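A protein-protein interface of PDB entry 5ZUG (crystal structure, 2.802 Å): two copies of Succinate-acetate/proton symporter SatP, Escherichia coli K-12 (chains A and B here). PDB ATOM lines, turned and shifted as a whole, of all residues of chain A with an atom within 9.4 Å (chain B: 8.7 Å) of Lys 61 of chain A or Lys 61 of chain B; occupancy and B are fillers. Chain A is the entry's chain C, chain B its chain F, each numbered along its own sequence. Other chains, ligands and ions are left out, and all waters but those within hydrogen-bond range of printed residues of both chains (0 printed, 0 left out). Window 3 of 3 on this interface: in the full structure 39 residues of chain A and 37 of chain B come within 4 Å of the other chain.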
ATOM      1  N   LYS A   7      -5.297 -26.173  13.593  1.00  0.00           N
ATOM      2  CA  LYS A   7      -4.826 -26.894  12.411  1.00  0.00           C
ATOM      3  C   LYS A   7      -3.327 -26.720  12.207  1.00  0.00           C
ATOM      4  O   LYS A   7      -2.687 -27.555  11.574  1.00  0.00           O
ATOM      5  CB  LYS A   7      -5.579 -26.463  11.150  1.00  0.00           C
ATOM      6  CG  LYS A   7      -5.233 -27.341   9.938  1.00  0.00           C
ATOM      7  CD  LYS A   7      -5.985 -26.929   8.688  1.00  0.00           C
ATOM      8  CE  LYS A   7      -7.453 -27.380   8.756  1.00  0.00           C
ATOM      9  NZ  LYS A   7      -8.335 -26.621   7.807  1.00  0.00           N
ATOM     10  N   LEU A   8      -2.781 -25.626  12.729  1.00  0.00           N
ATOM     11  CA  LEU A   8      -1.340 -25.433  12.788  1.00  0.00           C
ATOM     12  C   LEU A   8      -0.778 -26.222  13.966  1.00  0.00           C
ATOM     13  O   LEU A   8      -1.398 -26.272  15.032  1.00  0.00           O
ATOM     14  CB  LEU A   8      -1.013 -23.944  12.932  1.00  0.00           C
ATOM     15  CG  LEU A   8      -1.257 -23.007  11.740  1.00  0.00           C
ATOM     16  CD1 LEU A   8      -0.817 -21.580  12.064  1.00  0.00           C
ATOM     17  CD2 LEU A   8      -0.566 -23.467  10.481  1.00  0.00           C
ATOM     18  N   ALA A   9       0.371 -26.886  13.760  1.00  0.00           N
ATOM     19  CA  ALA A   9       1.004 -27.662  14.833  1.00  0.00           C
ATOM     20  C   ALA A   9       1.243 -26.791  16.072  1.00  0.00           C
ATOM     21  O   ALA A   9       1.310 -25.562  16.003  1.00  0.00           O
ATOM     22  CB  ALA A   9       2.319 -28.277  14.355  1.00  0.00           C
ATOM     23  N   PRO A  11       3.673 -25.341  18.669  1.00  0.00           N
ATOM     24  CA  PRO A  11       5.108 -25.142  18.887  1.00  0.00           C
ATOM     25  C   PRO A  11       5.549 -25.097  20.344  1.00  0.00           C
ATOM     26  O   PRO A  11       6.754 -24.899  20.593  1.00  0.00           O
ATOM     27  CB  PRO A  11       5.381 -23.806  18.185  1.00  0.00           C
ATOM     28  CG  PRO A  11       4.093 -23.054  18.282  1.00  0.00           C
ATOM     29  CD  PRO A  11       2.995 -24.096  18.245  1.00  0.00           C
ATOM     30  N   PHE A  54      12.557 -20.486  17.097  1.00  0.00           N
ATOM     31  CA  PHE A  54      11.607 -21.046  16.151  1.00  0.00           C
ATOM     32  C   PHE A  54      10.227 -21.183  16.790  1.00  0.00           C
ATOM     33  O   PHE A  54       9.240 -20.650  16.286  1.00  0.00           O
ATOM     34  CB  PHE A  54      12.114 -22.404  15.676  1.00  0.00           C
ATOM     35  CG  PHE A  54      13.291 -22.337  14.740  1.00  0.00           C
ATOM     36  CD1 PHE A  54      13.626 -21.169  14.083  1.00  0.00           C
ATOM     37  CD2 PHE A  54      14.036 -23.476  14.495  1.00  0.00           C
ATOM     38  CE1 PHE A  54      14.704 -21.138  13.209  1.00  0.00           C
ATOM     39  CE2 PHE A  54      15.096 -23.448  13.636  1.00  0.00           C
ATOM     40  CZ  PHE A  54      15.431 -22.275  12.981  1.00  0.00           C
ATOM     41  N   ALA A  55      10.163 -21.882  17.926  1.00  0.00           N
ATOM     42  CA  ALA A  55       8.915 -22.052  18.662  1.00  0.00           C
ATOM     43  C   ALA A  55       8.235 -20.716  18.926  1.00  0.00           C
ATOM     44  O   ALA A  55       7.021 -20.577  18.737  1.00  0.00           O
ATOM     45  CB  ALA A  55       9.183 -22.778  19.977  1.00  0.00           C
ATOM     46  N   GLY A  56       9.000 -19.717  19.354  1.00  0.00           N
ATOM     47  CA  GLY A  56       8.390 -18.429  19.617  1.00  0.00           C
ATOM     48  C   GLY A  56       7.791 -17.842  18.369  1.00  0.00           C
ATOM     49  O   GLY A  56       6.610 -17.504  18.343  1.00  0.00           O
ATOM     50  N   LEU A  57       8.555 -17.852  17.281  1.00  0.00           N
ATOM     51  CA  LEU A  57       8.044 -17.325  16.024  1.00  0.00           C
ATOM     52  C   LEU A  57       6.869 -18.145  15.495  1.00  0.00           C
ATOM     53  O   LEU A  57       6.043 -17.626  14.739  1.00  0.00           O
ATOM     54  CB  LEU A  57       9.151 -17.280  14.980  1.00  0.00           C
ATOM     55  CG  LEU A  57      10.375 -16.393  15.101  1.00  0.00           C
ATOM     56  CD1 LEU A  57      11.285 -16.698  13.915  1.00  0.00           C
ATOM     57  CD2 LEU A  57       9.994 -14.924  15.124  1.00  0.00           C
ATOM     58  N   LEU A  58       6.834 -19.442  15.786  1.00  0.00           N
ATOM     59  CA  LEU A  58       5.711 -20.250  15.357  1.00  0.00           C
ATOM     60  C   LEU A  58       4.439 -19.970  16.151  1.00  0.00           C
ATOM     61  O   LEU A  58       3.361 -20.438  15.740  1.00  0.00           O
ATOM     62  CB  LEU A  58       6.048 -21.730  15.421  1.00  0.00           C
ATOM     63  CG  LEU A  58       7.051 -22.253  14.409  1.00  0.00           C
ATOM     64  CD1 LEU A  58       7.221 -23.743  14.652  1.00  0.00           C
ATOM     65  CD2 LEU A  58       6.646 -21.953  12.991  1.00  0.00           C
ATOM     66  N   GLU A  59       4.545 -19.294  17.311  1.00  0.00           N
ATOM     67  CA  GLU A  59       3.343 -18.864  18.030  1.00  0.00           C
ATOM     68  C   GLU A  59       2.600 -17.707  17.349  1.00  0.00           C
ATOM     69  O   GLU A  59       1.449 -17.417  17.720  1.00  0.00           O
ATOM     70  CB  GLU A  59       3.699 -18.481  19.465  1.00  0.00           C
ATOM     71  CG  GLU A  59       4.134 -19.655  20.327  1.00  0.00           C
ATOM     72  CD  GLU A  59       3.036 -20.679  20.564  1.00  0.00           C
ATOM     73  OE1 GLU A  59       1.948 -20.551  19.972  1.00  0.00           O
ATOM     74  OE2 GLU A  59       3.249 -21.617  21.363  1.00  0.00           O
ATOM     75  N   TYR A  60       3.202 -17.088  16.332  1.00  0.00           N
ATOM     76  CA  TYR A  60       2.631 -15.900  15.711  1.00  0.00           C
ATOM     77  C   TYR A  60       1.415 -16.223  14.854  1.00  0.00           C
ATOM     78  O   TYR A  60       0.379 -15.558  14.955  1.00  0.00           O
ATOM     79  CB  TYR A  60       3.711 -15.242  14.883  1.00  0.00           C
ATOM     80  CG  TYR A  60       3.314 -14.104  14.011  1.00  0.00           C
ATOM     81  CD1 TYR A  60       3.064 -12.842  14.543  1.00  0.00           C
ATOM     82  CD2 TYR A  60       3.291 -14.253  12.645  1.00  0.00           C
ATOM     83  CE1 TYR A  60       2.749 -11.766  13.729  1.00  0.00           C
ATOM     84  CE2 TYR A  60       2.982 -13.199  11.823  1.00  0.00           C
ATOM     85  CZ  TYR A  60       2.714 -11.954  12.367  1.00  0.00           C
ATOM     86  OH  TYR A  60       2.412 -10.904  11.536  1.00  0.00           O
ATOM     87  N   LYS A  61       1.527 -17.198  13.957  1.00  0.00           N
ATOM     88  CA  LYS A  61       0.354 -17.513  13.144  1.00  0.00           C
ATOM     89  C   LYS A  61      -0.686 -18.269  13.949  1.00  0.00           C
ATOM     90  O   LYS A  61      -1.877 -18.170  13.655  1.00  0.00           O
ATOM     91  CB  LYS A  61       0.760 -18.273  11.889  1.00  0.00           C
ATOM     92  CG  LYS A  61       0.996 -17.338  10.710  1.00  0.00           C
ATOM     93  CD  LYS A  61       1.345 -18.102   9.451  1.00  0.00           C
ATOM     94  CE  LYS A  61       2.059 -17.224   8.427  1.00  0.00           C
ATOM     95  NZ  LYS A  61       2.788 -18.081   7.433  1.00  0.00           N
ATOM     96  N   LYS A  62      -0.274 -18.995  14.983  1.00  0.00           N
ATOM     97  CA  LYS A  62      -1.233 -19.330  16.023  1.00  0.00           C
ATOM     98  C   LYS A  62      -1.630 -18.038  16.739  1.00  0.00           C
ATOM     99  O   LYS A  62      -1.089 -16.963  16.471  1.00  0.00           O
ATOM    100  CB  LYS A  62      -0.652 -20.331  17.026  1.00  0.00           C
ATOM    101  CG  LYS A  62       0.100 -21.497  16.423  1.00  0.00           C
ATOM    102  CD  LYS A  62      -0.081 -22.756  17.280  1.00  0.00           C
ATOM    103  CE  LYS A  62      -1.348 -23.509  16.930  1.00  0.00           C
ATOM    104  NZ  LYS A  62      -1.500 -24.704  17.807  1.00  0.00           N
ATOM    105  N   GLY A  63      -2.599 -18.113  17.631  1.00  0.00           N
ATOM    106  CA  GLY A  63      -2.891 -16.772  18.117  1.00  0.00           C
ATOM    107  C   GLY A  63      -2.029 -16.219  19.240  1.00  0.00           C
ATOM    108  O   GLY A  63      -2.357 -15.146  19.761  1.00  0.00           O
ATOM    109  N   ASN A  64      -0.922 -16.887  19.591  1.00  0.00           N
ATOM    110  CA  ASN A  64      -0.363 -16.887  20.950  1.00  0.00           C
ATOM    111  C   ASN A  64       0.690 -15.805  21.195  1.00  0.00           C
ATOM    112  O   ASN A  64       1.890 -16.054  21.083  1.00  0.00           O
ATOM    113  CB  ASN A  64       0.176 -18.288  21.216  1.00  0.00           C
ATOM    114  CG  ASN A  64       0.448 -18.564  22.683  1.00  0.00           C
ATOM    115  OD1 ASN A  64       0.645 -17.649  23.493  1.00  0.00           O
ATOM    116  ND2 ASN A  64       0.403 -19.850  23.043  1.00  0.00           N
ATOM    117  N   THR A  65       0.243 -14.610  21.621  1.00  0.00           N
ATOM    118  CA  THR A  65       1.169 -13.517  21.961  1.00  0.00           C
ATOM    119  C   THR A  65       2.031 -13.851  23.176  1.00  0.00           C
ATOM    120  O   THR A  65       3.206 -13.462  23.242  1.00  0.00           O
ATOM    121  CB  THR A  65       0.410 -12.204  22.198  1.00  0.00           C
ATOM    122  OG1 THR A  65      -0.060 -11.692  20.947  1.00  0.00           O
ATOM    123  CG2 THR A  65       1.312 -11.151  22.828  1.00  0.00           C
ATOM    124  N   LEU A  68       4.592 -16.299  21.818  1.00  0.00           N
ATOM    125  CA  LEU A  68       5.504 -15.540  20.975  1.00  0.00           C
ATOM    126  C   LEU A  68       6.496 -14.761  21.816  1.00  0.00           C
ATOM    127  O   LEU A  68       7.709 -14.898  21.647  1.00  0.00           O
ATOM    128  CB  LEU A  68       4.758 -14.579  20.060  1.00  0.00           C
ATOM    129  CG  LEU A  68       5.748 -13.642  19.327  1.00  0.00           C
ATOM    130  CD1 LEU A  68       6.633 -14.405  18.376  1.00  0.00           C
ATOM    131  CD2 LEU A  68       5.057 -12.492  18.587  1.00  0.00           C
ATOM    132  N   LYS B   7      -6.076 -12.652  15.252  1.00  0.00           N
ATOM    133  CA  LYS B   7      -5.658 -14.043  15.198  1.00  0.00           C
ATOM    134  C   LYS B   7      -4.130 -14.143  15.090  1.00  0.00           C
ATOM    135  O   LYS B   7      -3.545 -15.162  15.478  1.00  0.00           O
ATOM    136  CB  LYS B   7      -6.333 -14.766  14.028  1.00  0.00           C
ATOM    137  CG  LYS B   7      -6.102 -16.290  14.012  1.00  0.00           C
ATOM    138  CD  LYS B   7      -6.778 -16.954  12.813  1.00  0.00           C
ATOM    139  CE  LYS B   7      -8.292 -17.013  13.012  1.00  0.00           C
ATOM    140  NZ  LYS B   7      -9.047 -17.230  11.743  1.00  0.00           N
ATOM    141  N   LEU B   8      -3.479 -13.117  14.532  1.00  0.00           N
ATOM    142  CA  LEU B   8      -2.022 -13.044  14.567  1.00  0.00           C
ATOM    143  C   LEU B   8      -1.567 -12.458  15.898  1.00  0.00           C
ATOM    144  O   LEU B   8      -2.065 -11.407  16.319  1.00  0.00           O
ATOM    145  CB  LEU B   8      -1.500 -12.185  13.416  1.00  0.00           C
ATOM    146  CG  LEU B   8      -1.587 -12.744  11.996  1.00  0.00           C
ATOM    147  CD1 LEU B   8      -0.940 -11.770  10.997  1.00  0.00           C
ATOM    148  CD2 LEU B   8      -0.961 -14.131  11.896  1.00  0.00           C
ATOM    149  N   ALA B   9      -0.594 -13.111  16.540  1.00  0.00           N
ATOM    150  CA  ALA B   9      -0.078 -12.646  17.822  1.00  0.00           C
ATOM    151  C   ALA B   9       0.449 -11.205  17.723  1.00  0.00           C
ATOM    152  O   ALA B   9       0.726 -10.676  16.640  1.00  0.00           O
ATOM    153  CB  ALA B   9       1.002 -13.599  18.336  1.00  0.00           C
ATOM    154  N   ASN B  10       0.541 -10.552  18.881  1.00  0.00           N
ATOM    155  CA  ASN B  10       1.075  -9.198  18.971  1.00  0.00           C
ATOM    156  C   ASN B  10       2.581  -9.267  19.168  1.00  0.00           C
ATOM    157  O   ASN B  10       3.029  -9.778  20.207  1.00  0.00           O
ATOM    158  CB  ASN B  10       0.429  -8.463  20.132  1.00  0.00           C
ATOM    159  CG  ASN B  10       0.744  -6.984  20.152  1.00  0.00           C
ATOM    160  OD1 ASN B  10       1.237  -6.416  19.178  1.00  0.00           O
ATOM    161  ND2 ASN B  10       0.434  -6.340  21.272  1.00  0.00           N
ATOM    162  N   PRO B  11       3.396  -8.785  18.217  1.00  0.00           N
ATOM    163  CA  PRO B  11       4.856  -8.815  18.396  1.00  0.00           C
ATOM    164  C   PRO B  11       5.431  -7.636  19.166  1.00  0.00           C
ATOM    165  O   PRO B  11       6.640  -7.647  19.449  1.00  0.00           O
ATOM    166  CB  PRO B  11       5.371  -8.808  16.947  1.00  0.00           C
ATOM    167  CG  PRO B  11       4.350  -8.007  16.206  1.00  0.00           C
ATOM    168  CD  PRO B  11       3.015  -8.284  16.880  1.00  0.00           C
ATOM    169  N   ALA B  55      10.286  -8.561  15.667  1.00  0.00           N
ATOM    170  CA  ALA B  55       9.081  -7.818  16.014  1.00  0.00           C
ATOM    171  C   ALA B  55       8.708  -6.851  14.906  1.00  0.00           C
ATOM    172  O   ALA B  55       7.566  -6.835  14.440  1.00  0.00           O
ATOM    173  CB  ALA B  55       9.288  -7.065  17.324  1.00  0.00           C
ATOM    174  N   GLY B  56       9.681  -6.095  14.409  1.00  0.00           N
ATOM    175  CA  GLY B  56       9.382  -5.162  13.338  1.00  0.00           C
ATOM    176  C   GLY B  56       8.870  -5.870  12.101  1.00  0.00           C
ATOM    177  O   GLY B  56       7.879  -5.451  11.495  1.00  0.00           O
ATOM    178  N   LEU B  57       9.524  -6.973  11.722  1.00  0.00           N
ATOM    179  CA  LEU B  57       9.064  -7.727  10.557  1.00  0.00           C
ATOM    180  C   LEU B  57       7.713  -8.397  10.804  1.00  0.00           C
ATOM    181  O   LEU B  57       6.898  -8.497   9.883  1.00  0.00           O
ATOM    182  CB  LEU B  57      10.104  -8.767  10.153  1.00  0.00           C
ATOM    183  CG  LEU B  57      11.412  -8.164   9.691  1.00  0.00           C
ATOM    184  CD1 LEU B  57      12.433  -9.251   9.388  1.00  0.00           C
ATOM    185  CD2 LEU B  57      11.128  -7.304   8.493  1.00  0.00           C
ATOM    186  N   LEU B  58       7.446  -8.871  12.026  1.00  0.00           N
ATOM    187  CA  LEU B  58       6.131  -9.467  12.269  1.00  0.00           C
ATOM    188  C   LEU B  58       4.986  -8.444  12.282  1.00  0.00           C
ATOM    189  O   LEU B  58       3.818  -8.843  12.295  1.00  0.00           O
ATOM    190  CB  LEU B  58       6.112 -10.288  13.566  1.00  0.00           C
ATOM    191  CG  LEU B  58       6.844 -11.631  13.578  1.00  0.00           C
ATOM    192  CD1 LEU B  58       6.735 -12.327  14.944  1.00  0.00           C
ATOM    193  CD2 LEU B  58       6.309 -12.517  12.480  1.00  0.00           C
ATOM    194  N   GLU B  59       5.287  -7.149  12.388  1.00  0.00           N
ATOM    195  CA  GLU B  59       4.265  -6.116  12.255  1.00  0.00           C
ATOM    196  C   GLU B  59       3.782  -5.949  10.821  1.00  0.00           C
ATOM    197  O   GLU B  59       2.759  -5.301  10.595  1.00  0.00           O
ATOM    198  CB  GLU B  59       4.796  -4.763  12.760  1.00  0.00           C
ATOM    199  CG  GLU B  59       5.076  -4.668  14.270  1.00  0.00           C
ATOM    200  CD  GLU B  59       3.842  -4.728  15.173  1.00  0.00           C
ATOM    201  OE1 GLU B  59       2.699  -4.958  14.697  1.00  0.00           O
ATOM    202  OE2 GLU B  59       4.026  -4.504  16.395  1.00  0.00           O
ATOM    203  N   TYR B  60       4.454  -6.557   9.857  1.00  0.00           N
ATOM    204  CA  TYR B  60       4.125  -6.311   8.460  1.00  0.00           C
ATOM    205  C   TYR B  60       2.805  -6.952   8.042  1.00  0.00           C
ATOM    206  O   TYR B  60       1.982  -6.305   7.389  1.00  0.00           O
ATOM    207  CB  TYR B  60       5.274  -6.804   7.601  1.00  0.00           C
ATOM    208  CG  TYR B  60       4.986  -6.885   6.144  1.00  0.00           C
ATOM    209  CD1 TYR B  60       4.966  -5.755   5.340  1.00  0.00           C
ATOM    210  CD2 TYR B  60       4.748  -8.115   5.567  1.00  0.00           C
ATOM    211  CE1 TYR B  60       4.712  -5.869   3.982  1.00  0.00           C
ATOM    212  CE2 TYR B  60       4.491  -8.232   4.249  1.00  0.00           C
ATOM    213  CZ  TYR B  60       4.476  -7.121   3.459  1.00  0.00           C
ATOM    214  OH  TYR B  60       4.235  -7.294   2.132  1.00  0.00           O
ATOM    215  N   LYS B  61       2.593  -8.231   8.359  1.00  0.00           N
ATOM    216  CA  LYS B  61       1.325  -8.856   7.970  1.00  0.00           C
ATOM    217  C   LYS B  61       0.164  -8.320   8.789  1.00  0.00           C
ATOM    218  O   LYS B  61      -0.984  -8.407   8.345  1.00  0.00           O
ATOM    219  CB  LYS B  61       1.408 -10.377   8.092  1.00  0.00           C
ATOM    220  CG  LYS B  61       1.816 -11.106   6.809  1.00  0.00           C
ATOM    221  CD  LYS B  61       1.875 -12.607   7.082  1.00  0.00           C
ATOM    222  CE  LYS B  61       2.756 -13.329   6.083  1.00  0.00           C
ATOM    223  NZ  LYS B  61       3.181 -14.645   6.638  1.00  0.00           N
ATOM    224  N   LYS B  62       0.438  -7.792   9.980  1.00  0.00           N
ATOM    225  CA  LYS B  62      -0.485  -6.886  10.642  1.00  0.00           C
ATOM    226  C   LYS B  62      -0.545  -5.575   9.851  1.00  0.00           C
ATOM    227  O   LYS B  62       0.181  -5.364   8.882  1.00  0.00           O
ATOM    228  CB  LYS B  62      -0.031  -6.614  12.075  1.00  0.00           C
ATOM    229  CG  LYS B  62       0.502  -7.846  12.786  1.00  0.00           C
ATOM    230  CD  LYS B  62       0.187  -7.858  14.280  1.00  0.00           C
ATOM    231  CE  LYS B  62      -1.183  -8.452  14.550  1.00  0.00           C
ATOM    232  NZ  LYS B  62      -1.456  -8.470  16.012  1.00  0.00           N
ATOM    233  N   GLY B  63      -1.433  -4.692  10.229  1.00  0.00           N
ATOM    234  CA  GLY B  63      -1.454  -3.538   9.345  1.00  0.00           C
ATOM    235  C   GLY B  63      -0.419  -2.475   9.632  1.00  0.00           C
ATOM    236  O   GLY B  63      -0.486  -1.387   9.050  1.00  0.00           O
ATOM    237  N   ASN B  64       0.552  -2.768  10.496  1.00  0.00           N
ATOM    238  CA  ASN B  64       1.234  -1.760  11.312  1.00  0.00           C
ATOM    239  C   ASN B  64       2.495  -1.185  10.672  1.00  0.00           C
ATOM    240  O   ASN B  64       3.597  -1.626  10.972  1.00  0.00           O
ATOM    241  CB  ASN B  64       1.563  -2.381  12.662  1.00  0.00           C
ATOM    242  CG  ASN B  64       1.894  -1.354  13.705  1.00  0.00           C
ATOM    243  OD1 ASN B  64       2.207  -0.200  13.384  1.00  0.00           O
ATOM    244  ND2 ASN B  64       1.821  -1.755  14.968  1.00  0.00           N
ATOM    245  N   THR B  65       2.357  -0.119   9.876  1.00  0.00           N
ATOM    246  CA  THR B  65       3.533   0.540   9.299  1.00  0.00           C
ATOM    247  C   THR B  65       4.432   1.159  10.370  1.00  0.00           C
ATOM    248  O   THR B  65       5.667   1.121  10.258  1.00  0.00           O
ATOM    249  CB  THR B  65       3.123   1.618   8.287  1.00  0.00           C
ATOM    250  OG1 THR B  65       2.651   1.009   7.075  1.00  0.00           O
ATOM    251  CG2 THR B  65       4.307   2.544   7.965  1.00  0.00           C
ATOM    252  N   LEU B  68       6.338  -1.643  12.128  1.00  0.00           N
ATOM    253  CA  LEU B  68       7.292  -2.128  11.138  1.00  0.00           C
ATOM    254  C   LEU B  68       8.513  -1.211  11.053  1.00  0.00           C
ATOM    255  O   LEU B  68       9.647  -1.654  11.247  1.00  0.00           O
ATOM    256  CB  LEU B  68       6.621  -2.260   9.769  1.00  0.00           C
ATOM    257  CG  LEU B  68       7.561  -2.641   8.611  1.00  0.00           C
ATOM    258  CD1 LEU B  68       8.140  -4.050   8.776  1.00  0.00           C
ATOM    259  CD2 LEU B  68       6.887  -2.500   7.247  1.00  0.00           C
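OH of Tyr 60 of chain A sits at hydrogen-bond distance from O of Leu 58 of chain B, at 2.6 Å.
The backbone carbonyl oxygen (O) of Lys 7 of chain B lies close to the backbone carbonyl oxygen (O) of Lys 62 of chain A (3.2 Å).
OG1 of Thr 65 of chain A sits at hydrogen-bond distance from N of Asn 10 of chain B, 2.4 Å away.
O of Tyr 60 of chain A lies within hydrogen-bond range of N of Ala 9 of chain B (3.1 Å).
N of Asn 64 of chain A is in hydrogen-bond range of O of Glu 59 of chain A, at 3.1 Å.
The backbone carbonyl oxygen (O) of Ala 9 of chain B lies within hydrogen-bond range of the side-chain amino group (NZ) of Lys 62 of chain B, at 3.2 Å.
The backbone carbonyl oxygen (O) of Ala 9 of chain A lies close to the side-chain amino group (NZ) of Lys 62 of chain A (3.4 Å).
O of Leu 8 of chain A lies within hydrogen-bond range of NZ of Lys 62 of chain A, 3.2 Å away.
The backbone carbonyl oxygen (O) of Leu 8 of chain B sits at hydrogen-bond distance from the side-chain amino group (NZ) of Lys 62 of chain B (3.0 Å).
Among the printed residues, pairs that only touch across the chains: Glu 59 of chain A with Ala 9 of chain B (3.9 Å), Tyr 60 of chain A with Lys 7 of chain B (3.98 Å), Tyr 60 of chain A with Leu 8 of chain B (3.5 Å), Tyr 60 of chain A with Lys 61 of chain B (3.6 Å), Tyr 60 of chain A with Lys 62 of chain B (3.8 Å), Lys 61 of chain A with Lys 7 of chain B (3.9 Å), Lys 61 of chain A with Leu 8 of chain B (3.8 Å), Lys 61 of chain A with Lys 61 of chain B (3.3 Å), Lys 62 of chain A with Ala 9 of chain B (3.9 Å), Gly 63 of chain A with Lys 7 of chain B (3.2 Å), Gly 63 of chain A with Ala 9 of chain B (3.9 Å), Asn 64 of chain A with Ala 9 of chain B (3.6 Å), Thr 65 of chain A with Ala 9 of chain B (3.3 Å), Leu 68 of chain A with Asn 10 of chain B (3.8 Å) and Leu 68 of chain A with Pro 11 of chain B (3.7 Å).
Ala 9 of chain A touches none of the printed residues of chain B.
Leu 57 of chain A touches none of the printed residues of chain B.
Of the printed residues of chain B, Leu 68 of chain A touches Asn 10 (3.8 Å) and Pro 11 (3.7 Å).
Printed residues of chain A within 4 Å of Leu 8 of chain B: Tyr 60 (3.5 Å) and Lys 61 (3.8 Å).
Lys 61 of chain B touches two residues of chain A.
The nearest residue of chain A that does not touch Lys 61 of chain B is Leu 57 of chain A (9.1 Å).
Hydrophobic or aromatic side chains of chain A within 4 Å of the printed part of chain B: Tyr 60 and Leu 68.
Printed residues of chain B that touch a printed residue of chain A: Lys 7, Leu 8, Ala 9, Asn 10, Pro 11, Leu 58, Lys 61 and Lys 62.
Among the printed residues, 19 pairs touch across the chains.
Among the printed residues, no Asp or Glu carboxylate lies within 4 Å of a Lys or Arg side-chain nitrogen of the other chain.
Tyr 60 of chain A touches Leu 58 of chain B, but with the chains exchanged Leu 58 of chain A does not touch Tyr 60 of chain B (14.4 Å).
Lys 61 of chain B touches its own counterpart, Lys 61 of chain A.
Lys 62 of chain A touches Ala 9 of chain B, but with the chains exchanged Ala 9 of chain A does not touch Lys 62 of chain B (17.3 Å).
Thr 65 of chain A touches Ala 9 of chain B, but with the chains exchanged Ala 9 of chain A does not touch Thr 65 of chain B (26.2 Å).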
